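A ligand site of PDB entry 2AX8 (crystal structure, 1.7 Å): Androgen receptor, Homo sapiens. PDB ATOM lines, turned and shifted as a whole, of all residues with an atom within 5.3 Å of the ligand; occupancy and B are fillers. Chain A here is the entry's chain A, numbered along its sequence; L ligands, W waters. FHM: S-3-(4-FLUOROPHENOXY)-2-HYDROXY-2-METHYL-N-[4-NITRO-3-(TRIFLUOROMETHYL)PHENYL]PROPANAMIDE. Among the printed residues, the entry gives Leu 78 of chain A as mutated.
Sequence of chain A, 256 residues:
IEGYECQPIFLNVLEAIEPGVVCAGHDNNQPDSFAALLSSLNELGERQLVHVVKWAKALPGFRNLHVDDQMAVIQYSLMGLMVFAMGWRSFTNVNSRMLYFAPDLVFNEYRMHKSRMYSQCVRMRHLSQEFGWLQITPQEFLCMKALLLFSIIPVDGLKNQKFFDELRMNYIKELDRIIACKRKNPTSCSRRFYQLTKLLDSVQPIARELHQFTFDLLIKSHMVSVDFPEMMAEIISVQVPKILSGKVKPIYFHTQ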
ATOM      1  N   LEU A  38     -12.068  -0.493 -19.687  1.00  0.00           N
ATOM      2  CA  LEU A  38     -13.299  -0.657 -20.441  1.00  0.00           C
ATOM      3  C   LEU A  38     -14.238   0.547 -20.322  1.00  0.00           C
ATOM      4  O   LEU A  38     -14.926   0.897 -21.287  1.00  0.00           O
ATOM      5  CB  LEU A  38     -14.010  -1.954 -20.040  1.00  0.00           C
ATOM      6  CG  LEU A  38     -13.672  -3.151 -20.951  1.00  0.00           C
ATOM      7  CD1 LEU A  38     -14.153  -2.872 -22.382  1.00  0.00           C
ATOM      8  CD2 LEU A  38     -12.170  -3.399 -20.943  1.00  0.00           C
ATOM      9  N   LEU A  41     -12.895   2.806 -22.830  1.00  0.00           N
ATOM     10  CA  LEU A  41     -13.154   2.385 -24.204  1.00  0.00           C
ATOM     11  C   LEU A  41     -14.600   2.748 -24.536  1.00  0.00           C
ATOM     12  O   LEU A  41     -14.882   3.208 -25.635  1.00  0.00           O
ATOM     13  CB  LEU A  41     -12.942   0.881 -24.378  1.00  0.00           C
ATOM     14  CG  LEU A  41     -11.490   0.410 -24.586  1.00  0.00           C
ATOM     15  CD1 LEU A  41     -11.431  -1.114 -24.580  1.00  0.00           C
ATOM     16  CD2 LEU A  41     -10.974   0.968 -25.910  1.00  0.00           C
ATOM     17  N   ASN A  42     -15.503   2.529 -23.588  1.00  0.00           N
ATOM     18  CA  ASN A  42     -16.927   2.847 -23.793  1.00  0.00           C
ATOM     19  C   ASN A  42     -17.145   4.341 -23.984  1.00  0.00           C
ATOM     20  O   ASN A  42     -17.890   4.755 -24.863  1.00  0.00           O
ATOM     21  CB  ASN A  42     -17.783   2.383 -22.603  1.00  0.00           C
ATOM     22  CG  ASN A  42     -17.891   0.881 -22.508  1.00  0.00           C
ATOM     23  OD1 ASN A  42     -17.573   0.147 -23.448  1.00  0.00           O
ATOM     24  ND2 ASN A  42     -18.362   0.399 -21.356  1.00  0.00           N
ATOM     25  N   LEU A  44     -14.898   6.493 -24.934  1.00  0.00           N
ATOM     26  CA  LEU A  44     -14.242   6.869 -26.185  1.00  0.00           C
ATOM     27  C   LEU A  44     -15.188   6.520 -27.348  1.00  0.00           C
ATOM     28  O   LEU A  44     -15.278   7.266 -28.318  1.00  0.00           O
ATOM     29  CB  LEU A  44     -12.914   6.116 -26.370  1.00  0.00           C
ATOM     30  CG  LEU A  44     -12.160   6.390 -27.681  1.00  0.00           C
ATOM     31  CD1 LEU A  44     -11.905   7.898 -27.827  1.00  0.00           C
ATOM     32  CD2 LEU A  44     -10.841   5.628 -27.685  1.00  0.00           C
ATOM     33  N   GLY A  45     -15.872   5.379 -27.234  1.00  0.00           N
ATOM     34  CA  GLY A  45     -16.814   4.971 -28.264  1.00  0.00           C
ATOM     35  C   GLY A  45     -17.937   5.979 -28.401  1.00  0.00           C
ATOM     36  O   GLY A  45     -18.330   6.349 -29.514  1.00  0.00           O
ATOM     37  N   GLN A  48     -16.452   9.023 -30.139  1.00  0.00           N
ATOM     38  CA  GLN A  48     -16.204   8.785 -31.560  1.00  0.00           C
ATOM     39  C   GLN A  48     -17.528   8.706 -32.339  1.00  0.00           C
ATOM     40  O   GLN A  48     -17.607   9.182 -33.476  1.00  0.00           O
ATOM     41  CB  GLN A  48     -15.372   7.513 -31.758  1.00  0.00           C
ATOM     42  CG  GLN A  48     -13.949   7.656 -31.172  1.00  0.00           C
ATOM     43  CD  GLN A  48     -13.020   6.505 -31.524  1.00  0.00           C
ATOM     44  OE1 GLN A  48     -11.826   6.523 -31.184  1.00  0.00           O
ATOM     45  NE2 GLN A  48     -13.548   5.492 -32.208  1.00  0.00           N
ATOM     46  N   GLN A  75     -25.076   3.031 -37.437  1.00  0.00           N
ATOM     47  CA  GLN A  75     -24.998   2.189 -36.256  1.00  0.00           C
ATOM     48  C   GLN A  75     -24.504   0.774 -36.542  1.00  0.00           C
ATOM     49  O   GLN A  75     -23.693   0.236 -35.794  1.00  0.00           O
ATOM     50  CB  GLN A  75     -26.360   2.177 -35.545  1.00  0.00           C
ATOM     51  CG  GLN A  75     -26.824   3.582 -35.187  1.00  0.00           C
ATOM     52  CD  GLN A  75     -28.151   3.632 -34.451  1.00  0.00           C
ATOM     53  OE1 GLN A  75     -29.070   2.871 -34.752  1.00  0.00           O
ATOM     54  NE2 GLN A  75     -28.263   4.548 -33.497  1.00  0.00           N
ATOM     55  N   LEU A  78     -20.754   1.130 -37.472  1.00  0.00           N
ATOM     56  CA  LEU A  78     -19.922   1.836 -36.498  1.00  0.00           C
ATOM     57  C   LEU A  78     -18.645   1.126 -36.046  1.00  0.00           C
ATOM     58  O   LEU A  78     -17.540   1.670 -36.177  1.00  0.00           O
ATOM     59  CB  LEU A  78     -20.752   2.212 -35.265  1.00  0.00           C
ATOM     60  CG  LEU A  78     -19.977   3.005 -34.203  1.00  0.00           C
ATOM     61  CD1 LEU A  78     -19.465   4.313 -34.801  1.00  0.00           C
ATOM     62  CD2 LEU A  78     -20.883   3.284 -33.008  1.00  0.00           C
ATOM     63  N   MET A  79     -18.785  -0.078 -35.493  1.00  0.00           N
ATOM     64  CA  MET A  79     -17.634  -0.838 -35.005  1.00  0.00           C
ATOM     65  C   MET A  79     -16.590  -1.028 -36.093  1.00  0.00           C
ATOM     66  O   MET A  79     -15.397  -0.805 -35.866  1.00  0.00           O
ATOM     67  CB  MET A  79     -18.077  -2.204 -34.459  1.00  0.00           C
ATOM     68  CG  MET A  79     -16.955  -3.018 -33.783  1.00  0.00           C
ATOM     69  SD  MET A  79     -16.277  -2.227 -32.280  1.00  0.00           S
ATOM     70  CE  MET A  79     -17.465  -2.786 -31.044  1.00  0.00           C
ATOM     71  N   MET A  82     -14.776   2.193 -36.801  1.00  0.00           N
ATOM     72  CA  MET A  82     -13.859   2.512 -35.730  1.00  0.00           C
ATOM     73  C   MET A  82     -12.596   1.651 -35.796  1.00  0.00           C
ATOM     74  O   MET A  82     -11.483   2.151 -35.630  1.00  0.00           O
ATOM     75  CB  MET A  82     -14.561   2.353 -34.381  1.00  0.00           C
ATOM     76  CG  MET A  82     -15.601   3.446 -34.117  1.00  0.00           C
ATOM     77  SD  MET A  82     -16.671   3.070 -32.701  1.00  0.00           S
ATOM     78  CE  MET A  82     -15.478   3.000 -31.388  1.00  0.00           C
ATOM     79  N   VAL A  83     -12.784   0.352 -36.045  1.00  0.00           N
ATOM     80  CA  VAL A  83     -11.660  -0.573 -36.136  1.00  0.00           C
ATOM     81  C   VAL A  83     -10.690  -0.184 -37.248  1.00  0.00           C
ATOM     82  O   VAL A  83      -9.471  -0.183 -37.047  1.00  0.00           O
ATOM     83  CB  VAL A  83     -12.163  -2.024 -36.407  1.00  0.00           C
ATOM     84  CG1 VAL A  83     -11.002  -2.922 -36.804  1.00  0.00           C
ATOM     85  CG2 VAL A  83     -12.854  -2.584 -35.154  1.00  0.00           C
ATOM     86  N   MET A  86      -8.831   3.064 -36.333  1.00  0.00           N
ATOM     87  CA  MET A  86      -7.881   2.823 -35.253  1.00  0.00           C
ATOM     88  C   MET A  86      -6.651   2.099 -35.800  1.00  0.00           C
ATOM     89  O   MET A  86      -5.533   2.413 -35.417  1.00  0.00           O
ATOM     90  CB  MET A  86      -8.535   1.995 -34.134  1.00  0.00           C
ATOM     91  CG  MET A  86      -7.738   1.941 -32.833  1.00  0.00           C
ATOM     92  SD  MET A  86      -6.469   0.663 -32.836  1.00  0.00           S
ATOM     93  CE  MET A  86      -7.472  -0.799 -32.516  1.00  0.00           C
ATOM     94  N   ARG A  89      -4.504   4.658 -37.447  1.00  0.00           N
ATOM     95  CA  ARG A  89      -3.817   5.490 -36.450  1.00  0.00           C
ATOM     96  C   ARG A  89      -2.625   4.744 -35.837  1.00  0.00           C
ATOM     97  O   ARG A  89      -1.560   5.317 -35.625  1.00  0.00           O
ATOM     98  CB  ARG A  89      -4.768   5.922 -35.333  1.00  0.00           C
ATOM     99  CG  ARG A  89      -5.806   6.960 -35.724  1.00  0.00           C
ATOM    100  CD  ARG A  89      -6.462   7.586 -34.498  1.00  0.00           C
ATOM    101  NE  ARG A  89      -7.198   6.617 -33.678  1.00  0.00           N
ATOM    102  CZ  ARG A  89      -8.432   6.198 -33.945  1.00  0.00           C
ATOM    103  NH1 ARG A  89      -9.085   6.650 -35.008  1.00  0.00           N
ATOM    104  NH2 ARG A  89      -9.017   5.310 -33.144  1.00  0.00           N
ATOM    105  N   PHE A 101      -5.875   3.643 -29.756  1.00  0.00           N
ATOM    106  CA  PHE A 101      -7.319   3.928 -29.693  1.00  0.00           C
ATOM    107  C   PHE A 101      -7.506   5.437 -29.656  1.00  0.00           C
ATOM    108  O   PHE A 101      -8.407   5.980 -30.298  1.00  0.00           O
ATOM    109  CB  PHE A 101      -7.956   3.303 -28.460  1.00  0.00           C
ATOM    110  CG  PHE A 101      -8.010   1.802 -28.489  1.00  0.00           C
ATOM    111  CD1 PHE A 101      -6.961   1.043 -27.988  1.00  0.00           C
ATOM    112  CD2 PHE A 101      -9.108   1.150 -29.038  1.00  0.00           C
ATOM    113  CE1 PHE A 101      -7.006  -0.354 -28.023  1.00  0.00           C
ATOM    114  CE2 PHE A 101      -9.160  -0.247 -29.080  1.00  0.00           C
ATOM    115  CZ  PHE A 101      -8.111  -1.005 -28.578  1.00  0.00           C
ATOM    116  N   MET A 117      -9.687  -8.465 -24.097  1.00  0.00           N
ATOM    117  CA  MET A 117     -10.001  -8.341 -25.517  1.00  0.00           C
ATOM    118  C   MET A 117      -8.724  -8.667 -26.284  1.00  0.00           C
ATOM    119  O   MET A 117      -8.506  -8.148 -27.383  1.00  0.00           O
ATOM    120  CB  MET A 117     -10.389  -6.893 -25.850  1.00  0.00           C
ATOM    121  CG  MET A 117     -11.434  -6.299 -24.940  1.00  0.00           C
ATOM    122  SD  MET A 117     -11.652  -4.543 -25.272  1.00  0.00           S
ATOM    123  CE  MET A 117     -12.461  -4.606 -26.829  1.00  0.00           C
ATOM    124  N   MET A 124      -6.395  -6.664 -34.622  1.00  0.00           N
ATOM    125  CA  MET A 124      -6.385  -5.278 -35.058  1.00  0.00           C
ATOM    126  C   MET A 124      -4.934  -4.828 -35.232  1.00  0.00           C
ATOM    127  O   MET A 124      -4.635  -3.973 -36.068  1.00  0.00           O
ATOM    128  CB  MET A 124      -7.116  -4.381 -34.054  1.00  0.00           C
ATOM    129  CG  MET A 124      -8.610  -4.697 -33.945  1.00  0.00           C
ATOM    130  SD  MET A 124      -9.577  -3.470 -33.048  1.00  0.00           S
ATOM    131  CE  MET A 124      -9.151  -3.872 -31.357  1.00  0.00           C
ATOM    132  N   LEU A 210     -15.614  -8.138 -31.684  1.00  0.00           N
ATOM    133  CA  LEU A 210     -15.752  -7.044 -30.735  1.00  0.00           C
ATOM    134  C   LEU A 210     -17.216  -6.904 -30.344  1.00  0.00           C
ATOM    135  O   LEU A 210     -17.542  -6.663 -29.171  1.00  0.00           O
ATOM    136  CB  LEU A 210     -15.238  -5.747 -31.368  1.00  0.00           C
ATOM    137  CG  LEU A 210     -13.706  -5.696 -31.457  1.00  0.00           C
ATOM    138  CD1 LEU A 210     -13.257  -4.560 -32.363  1.00  0.00           C
ATOM    139  CD2 LEU A 210     -13.136  -5.519 -30.045  1.00  0.00           C
ATOM    140  N   HIS A 211     -18.108  -7.064 -31.327  1.00  0.00           N
ATOM    141  CA  HIS A 211     -19.539  -6.985 -31.072  1.00  0.00           C
ATOM    142  C   HIS A 211     -19.961  -8.027 -30.039  1.00  0.00           C
ATOM    143  O   HIS A 211     -20.729  -7.734 -29.131  1.00  0.00           O
ATOM    144  CB  HIS A 211     -20.320  -7.215 -32.361  1.00  0.00           C
ATOM    145  CG  HIS A 211     -20.509  -5.974 -33.189  1.00  0.00           C
ATOM    146  ND1 HIS A 211     -20.623  -6.003 -34.559  1.00  0.00           N
ATOM    147  CD2 HIS A 211     -20.642  -4.676 -32.824  1.00  0.00           C
ATOM    148  CE1 HIS A 211     -20.819  -4.776 -35.007  1.00  0.00           C
ATOM    149  NE2 HIS A 211     -20.830  -3.954 -33.974  1.00  0.00           N
ATOM    150  N   PHE A 213     -18.025  -9.553 -27.774  1.00  0.00           N
ATOM    151  CA  PHE A 213     -17.418  -9.212 -26.506  1.00  0.00           C
ATOM    152  C   PHE A 213     -18.190  -8.086 -25.829  1.00  0.00           C
ATOM    153  O   PHE A 213     -18.510  -8.159 -24.649  1.00  0.00           O
ATOM    154  CB  PHE A 213     -15.956  -8.796 -26.710  1.00  0.00           C
ATOM    155  CG  PHE A 213     -15.343  -8.113 -25.524  1.00  0.00           C
ATOM    156  CD1 PHE A 213     -15.431  -6.731 -25.379  1.00  0.00           C
ATOM    157  CD2 PHE A 213     -14.664  -8.849 -24.553  1.00  0.00           C
ATOM    158  CE1 PHE A 213     -14.858  -6.092 -24.272  1.00  0.00           C
ATOM    159  CE2 PHE A 213     -14.094  -8.220 -23.443  1.00  0.00           C
ATOM    160  CZ  PHE A 213     -14.190  -6.837 -23.305  1.00  0.00           C
ATOM    161  N   THR A 214     -18.479  -7.036 -26.595  1.00  0.00           N
ATOM    162  CA  THR A 214     -19.197  -5.881 -26.057  1.00  0.00           C
ATOM    163  C   THR A 214     -20.601  -6.248 -25.594  1.00  0.00           C
ATOM    164  O   THR A 214     -21.058  -5.789 -24.548  1.00  0.00           O
ATOM    165  CB  THR A 214     -19.259  -4.749 -27.087  1.00  0.00           C
ATOM    166  OG1 THR A 214     -17.930  -4.419 -27.494  1.00  0.00           O
ATOM    167  CG2 THR A 214     -19.922  -3.520 -26.503  1.00  0.00           C
ATOM    168  N   LEU A 217     -20.370  -8.091 -22.383  1.00  0.00           N
ATOM    169  CA  LEU A 217     -19.969  -7.165 -21.321  1.00  0.00           C
ATOM    170  C   LEU A 217     -21.161  -6.332 -20.844  1.00  0.00           C
ATOM    171  O   LEU A 217     -21.360  -6.163 -19.639  1.00  0.00           O
ATOM    172  CB  LEU A 217     -18.834  -6.255 -21.795  1.00  0.00           C
ATOM    173  CG  LEU A 217     -18.225  -5.326 -20.732  1.00  0.00           C
ATOM    174  CD1 LEU A 217     -17.828  -6.130 -19.506  1.00  0.00           C
ATOM    175  CD2 LEU A 217     -17.025  -4.595 -21.307  1.00  0.00           C
ATOM    176  N   MET A 232     -24.214   4.223 -26.570  1.00  0.00           N
ATOM    177  CA  MET A 232     -23.540   2.942 -26.738  1.00  0.00           C
ATOM    178  C   MET A 232     -24.479   1.829 -26.274  1.00  0.00           C
ATOM    179  O   MET A 232     -24.663   0.828 -26.976  1.00  0.00           O
ATOM    180  CB  MET A 232     -22.261   2.912 -25.896  1.00  0.00           C
ATOM    181  CG  MET A 232     -21.143   3.819 -26.396  1.00  0.00           C
ATOM    182  SD  MET A 232     -20.359   3.198 -27.913  1.00  0.00           S
ATOM    183  CE  MET A 232     -21.284   4.120 -29.159  1.00  0.00           C
ATOM    184  N   ILE A 235     -27.256   1.185 -28.865  1.00  0.00           N
ATOM    185  CA  ILE A 235     -26.768   0.490 -30.052  1.00  0.00           C
ATOM    186  C   ILE A 235     -26.449  -0.983 -29.762  1.00  0.00           C
ATOM    187  O   ILE A 235     -26.821  -1.862 -30.530  1.00  0.00           O
ATOM    188  CB  ILE A 235     -25.506   1.181 -30.625  1.00  0.00           C
ATOM    189  CG1 ILE A 235     -25.908   2.496 -31.305  1.00  0.00           C
ATOM    190  CG2 ILE A 235     -24.805   0.261 -31.626  1.00  0.00           C
ATOM    191  CD1 ILE A 235     -24.725   3.309 -31.841  1.00  0.00           C
ATOM    192  N   ILE A 236     -25.799  -1.242 -28.638  1.00  0.00           N
ATOM    193  CA  ILE A 236     -25.417  -2.599 -28.261  1.00  0.00           C
ATOM    194  C   ILE A 236     -26.624  -3.498 -27.965  1.00  0.00           C
ATOM    195  O   ILE A 236     -26.608  -4.681 -28.278  1.00  0.00           O
ATOM    196  CB  ILE A 236     -24.519  -2.608 -27.000  1.00  0.00           C
ATOM    197  CG1 ILE A 236     -23.248  -1.795 -27.267  1.00  0.00           C
ATOM    198  CG2 ILE A 236     -24.161  -4.042 -26.614  1.00  0.00           C
ATOM    199  CD1 ILE A 236     -22.422  -1.530 -26.030  1.00  0.00           C
ATOM    200  N   VAL A 240     -26.796  -4.185 -32.323  1.00  0.00           N
ATOM    201  CA  VAL A 240     -25.804  -5.264 -32.297  1.00  0.00           C
ATOM    202  C   VAL A 240     -26.412  -6.671 -32.271  1.00  0.00           C
ATOM    203  O   VAL A 240     -25.891  -7.584 -32.920  1.00  0.00           O
ATOM    204  CB  VAL A 240     -24.823  -5.091 -31.108  1.00  0.00           C
ATOM    205  CG1 VAL A 240     -23.923  -6.321 -30.950  1.00  0.00           C
ATOM    206  CG2 VAL A 240     -23.960  -3.831 -31.335  1.00  0.00           C
HETATM  207  C17 FHM L   1     -19.932  -0.665 -29.085  1.00  0.00           C
HETATM  208  C18 FHM L   1     -20.793  -0.830 -30.167  1.00  0.00           C
HETATM  209  C19 FHM L   1     -20.467  -0.300 -31.408  1.00  0.00           C
HETATM  210  F19 FHM L   1     -21.297  -0.463 -32.450  1.00  0.00           F
HETATM  211  C20 FHM L   1     -19.269   0.405 -31.564  1.00  0.00           C
HETATM  212  C21 FHM L   1     -18.415   0.570 -30.489  1.00  0.00           C
HETATM  213  C16 FHM L   1     -18.734   0.040 -29.241  1.00  0.00           C
HETATM  214  O14 FHM L   1     -17.869   0.222 -28.209  1.00  0.00           O
HETATM  215  C13 FHM L   1     -17.709  -0.901 -27.341  1.00  0.00           C
HETATM  216  C11 FHM L   1     -16.353  -0.780 -26.644  1.00  0.00           C
HETATM  217  O11 FHM L   1     -16.364   0.384 -25.811  1.00  0.00           O
HETATM  218  C12 FHM L   1     -16.081  -2.037 -25.823  1.00  0.00           C
HETATM  219  C10 FHM L   1     -15.283  -0.598 -27.730  1.00  0.00           C
HETATM  220  O10 FHM L   1     -14.973  -1.530 -28.471  1.00  0.00           O
HETATM  221  N9  FHM L   1     -14.763   0.625 -27.770  1.00  0.00           N
HETATM  222  C6  FHM L   1     -13.838   1.044 -28.641  1.00  0.00           C
HETATM  223  C5  FHM L   1     -13.406   0.269 -29.719  1.00  0.00           C
HETATM  224  C1  FHM L   1     -13.408   2.358 -28.539  1.00  0.00           C
HETATM  225  C2  FHM L   1     -12.568   2.879 -29.520  1.00  0.00           C
HETATM  226  C3  FHM L   1     -12.158   2.108 -30.604  1.00  0.00           C
HETATM  227  N8  FHM L   1     -11.394   2.729 -31.506  1.00  0.00           N
HETATM  228  O2  FHM L   1     -11.118   2.176 -32.790  1.00  0.00           O
HETATM  229  O1  FHM L   1     -10.981   4.064 -31.274  1.00  0.00           O
HETATM  230  C4  FHM L   1     -12.557   0.772 -30.712  1.00  0.00           C
HETATM  231  C7  FHM L   1     -12.051  -0.190 -31.795  1.00  0.00           C
HETATM  232  F2  FHM L   1     -12.705   0.011 -32.932  1.00  0.00           F
HETATM  233  F3  FHM L   1     -10.745  -0.052 -32.031  1.00  0.00           F
HETATM  234  F1  FHM L   1     -12.209  -1.464 -31.457  1.00  0.00           F
HETATM  235  O   HOH W   1     -11.659   4.797 -34.432  1.00  0.00           O
HETATM  236  O   HOH W   2     -21.524  -1.385 -35.252  1.00  0.00           O
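O11 of the ligand is in hydrogen-bond range of O of Leu 41 (3.2 Å). O11 of the ligand lies within hydrogen-bond range of N of Asn 42, 3.2 Å away. The side-chain amide oxygen (OE1) of Gln 48 lies close to an oxygen (O1) of the ligand. OD1 of Asn 42 lies within hydrogen-bond range of O11 of the ligand (2.7 Å). NH2 of Arg 89 lies within hydrogen-bond range of O1 of the ligand (3.0 Å).
An oxygen (O2) of the ligand sits close to the backbone carbonyl oxygen of Met 82, at 2.9 Å. The backbone NH (N) of Val 83 lies close to a fluorine (F2) of the ligand, 3.1 Å away. The backbone carbonyl oxygen (O) of Phe 101 lies close to an oxygen (O1) of the ligand (3.4 Å). The side-chain sulfur (SD) of Met 124 sits close to a fluorine (F1) of the ligand, at 3.7 Å. Merely in contact with the ligand: Leu 44, Leu 78, Met 79, Met 86, Leu 210, His 211, Thr 214, Met 232, Ile 235 and Ile 236. Hydrophobic or aromatic side chains within 4 Å of the ligand: Leu 41, Leu 44, Leu 78, Met 79, Met 82, Val 83, Met 86, Phe 101, Met 124, Leu 210, Met 232, Ile 235 and Ile 236. 18 residues have an atom within 4 Å of the ligand: Leu 41, Asn 42, Leu 44, Gln 48, Leu 78, Met 79, Met 82, Val 83, Met 86, Arg 89, Phe 101, Met 124, Leu 210, His 211, Thr 214, Met 232, Ile 235 and Ile 236. The nearest printed residue that does not touch the ligand is Leu 38 (4.03 Å).
The side-chain hydroxyl (OG1) of Thr 214 is in hydrogen-bond range of the backbone carbonyl oxygen (O) of Leu 210. The guanidinium group (NH2) of Arg 89 sits at hydrogen-bond distance from the backbone carbonyl oxygen (O) of Phe 101 (3.0 Å). O of Ile 235 sits at hydrogen-bond distance from N of Val 240 (2.9 Å). ND2 of Asn 42 lies close to O of Leu 38 (3.5 Å).
Water W2 lies within hydrogen-bond range of the backbone carbonyl oxygen of Gln 75 (2.8 Å), a ring nitrogen (NE2) of His 211 (3.0 Å), the backbone NH of Met 79 (3.0 Å) and the backbone NH of Leu 78 (3.4 Å). Water W1 lies within hydrogen-bond range of the backbone carbonyl oxygen of Met 82 (2.9 Å), the guanidinium group of Arg 89 (3.0 Å), the side-chain amide nitrogen of Gln 48 (3.0 Å) and an oxygen (O2) of the ligand (3.1 Å).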
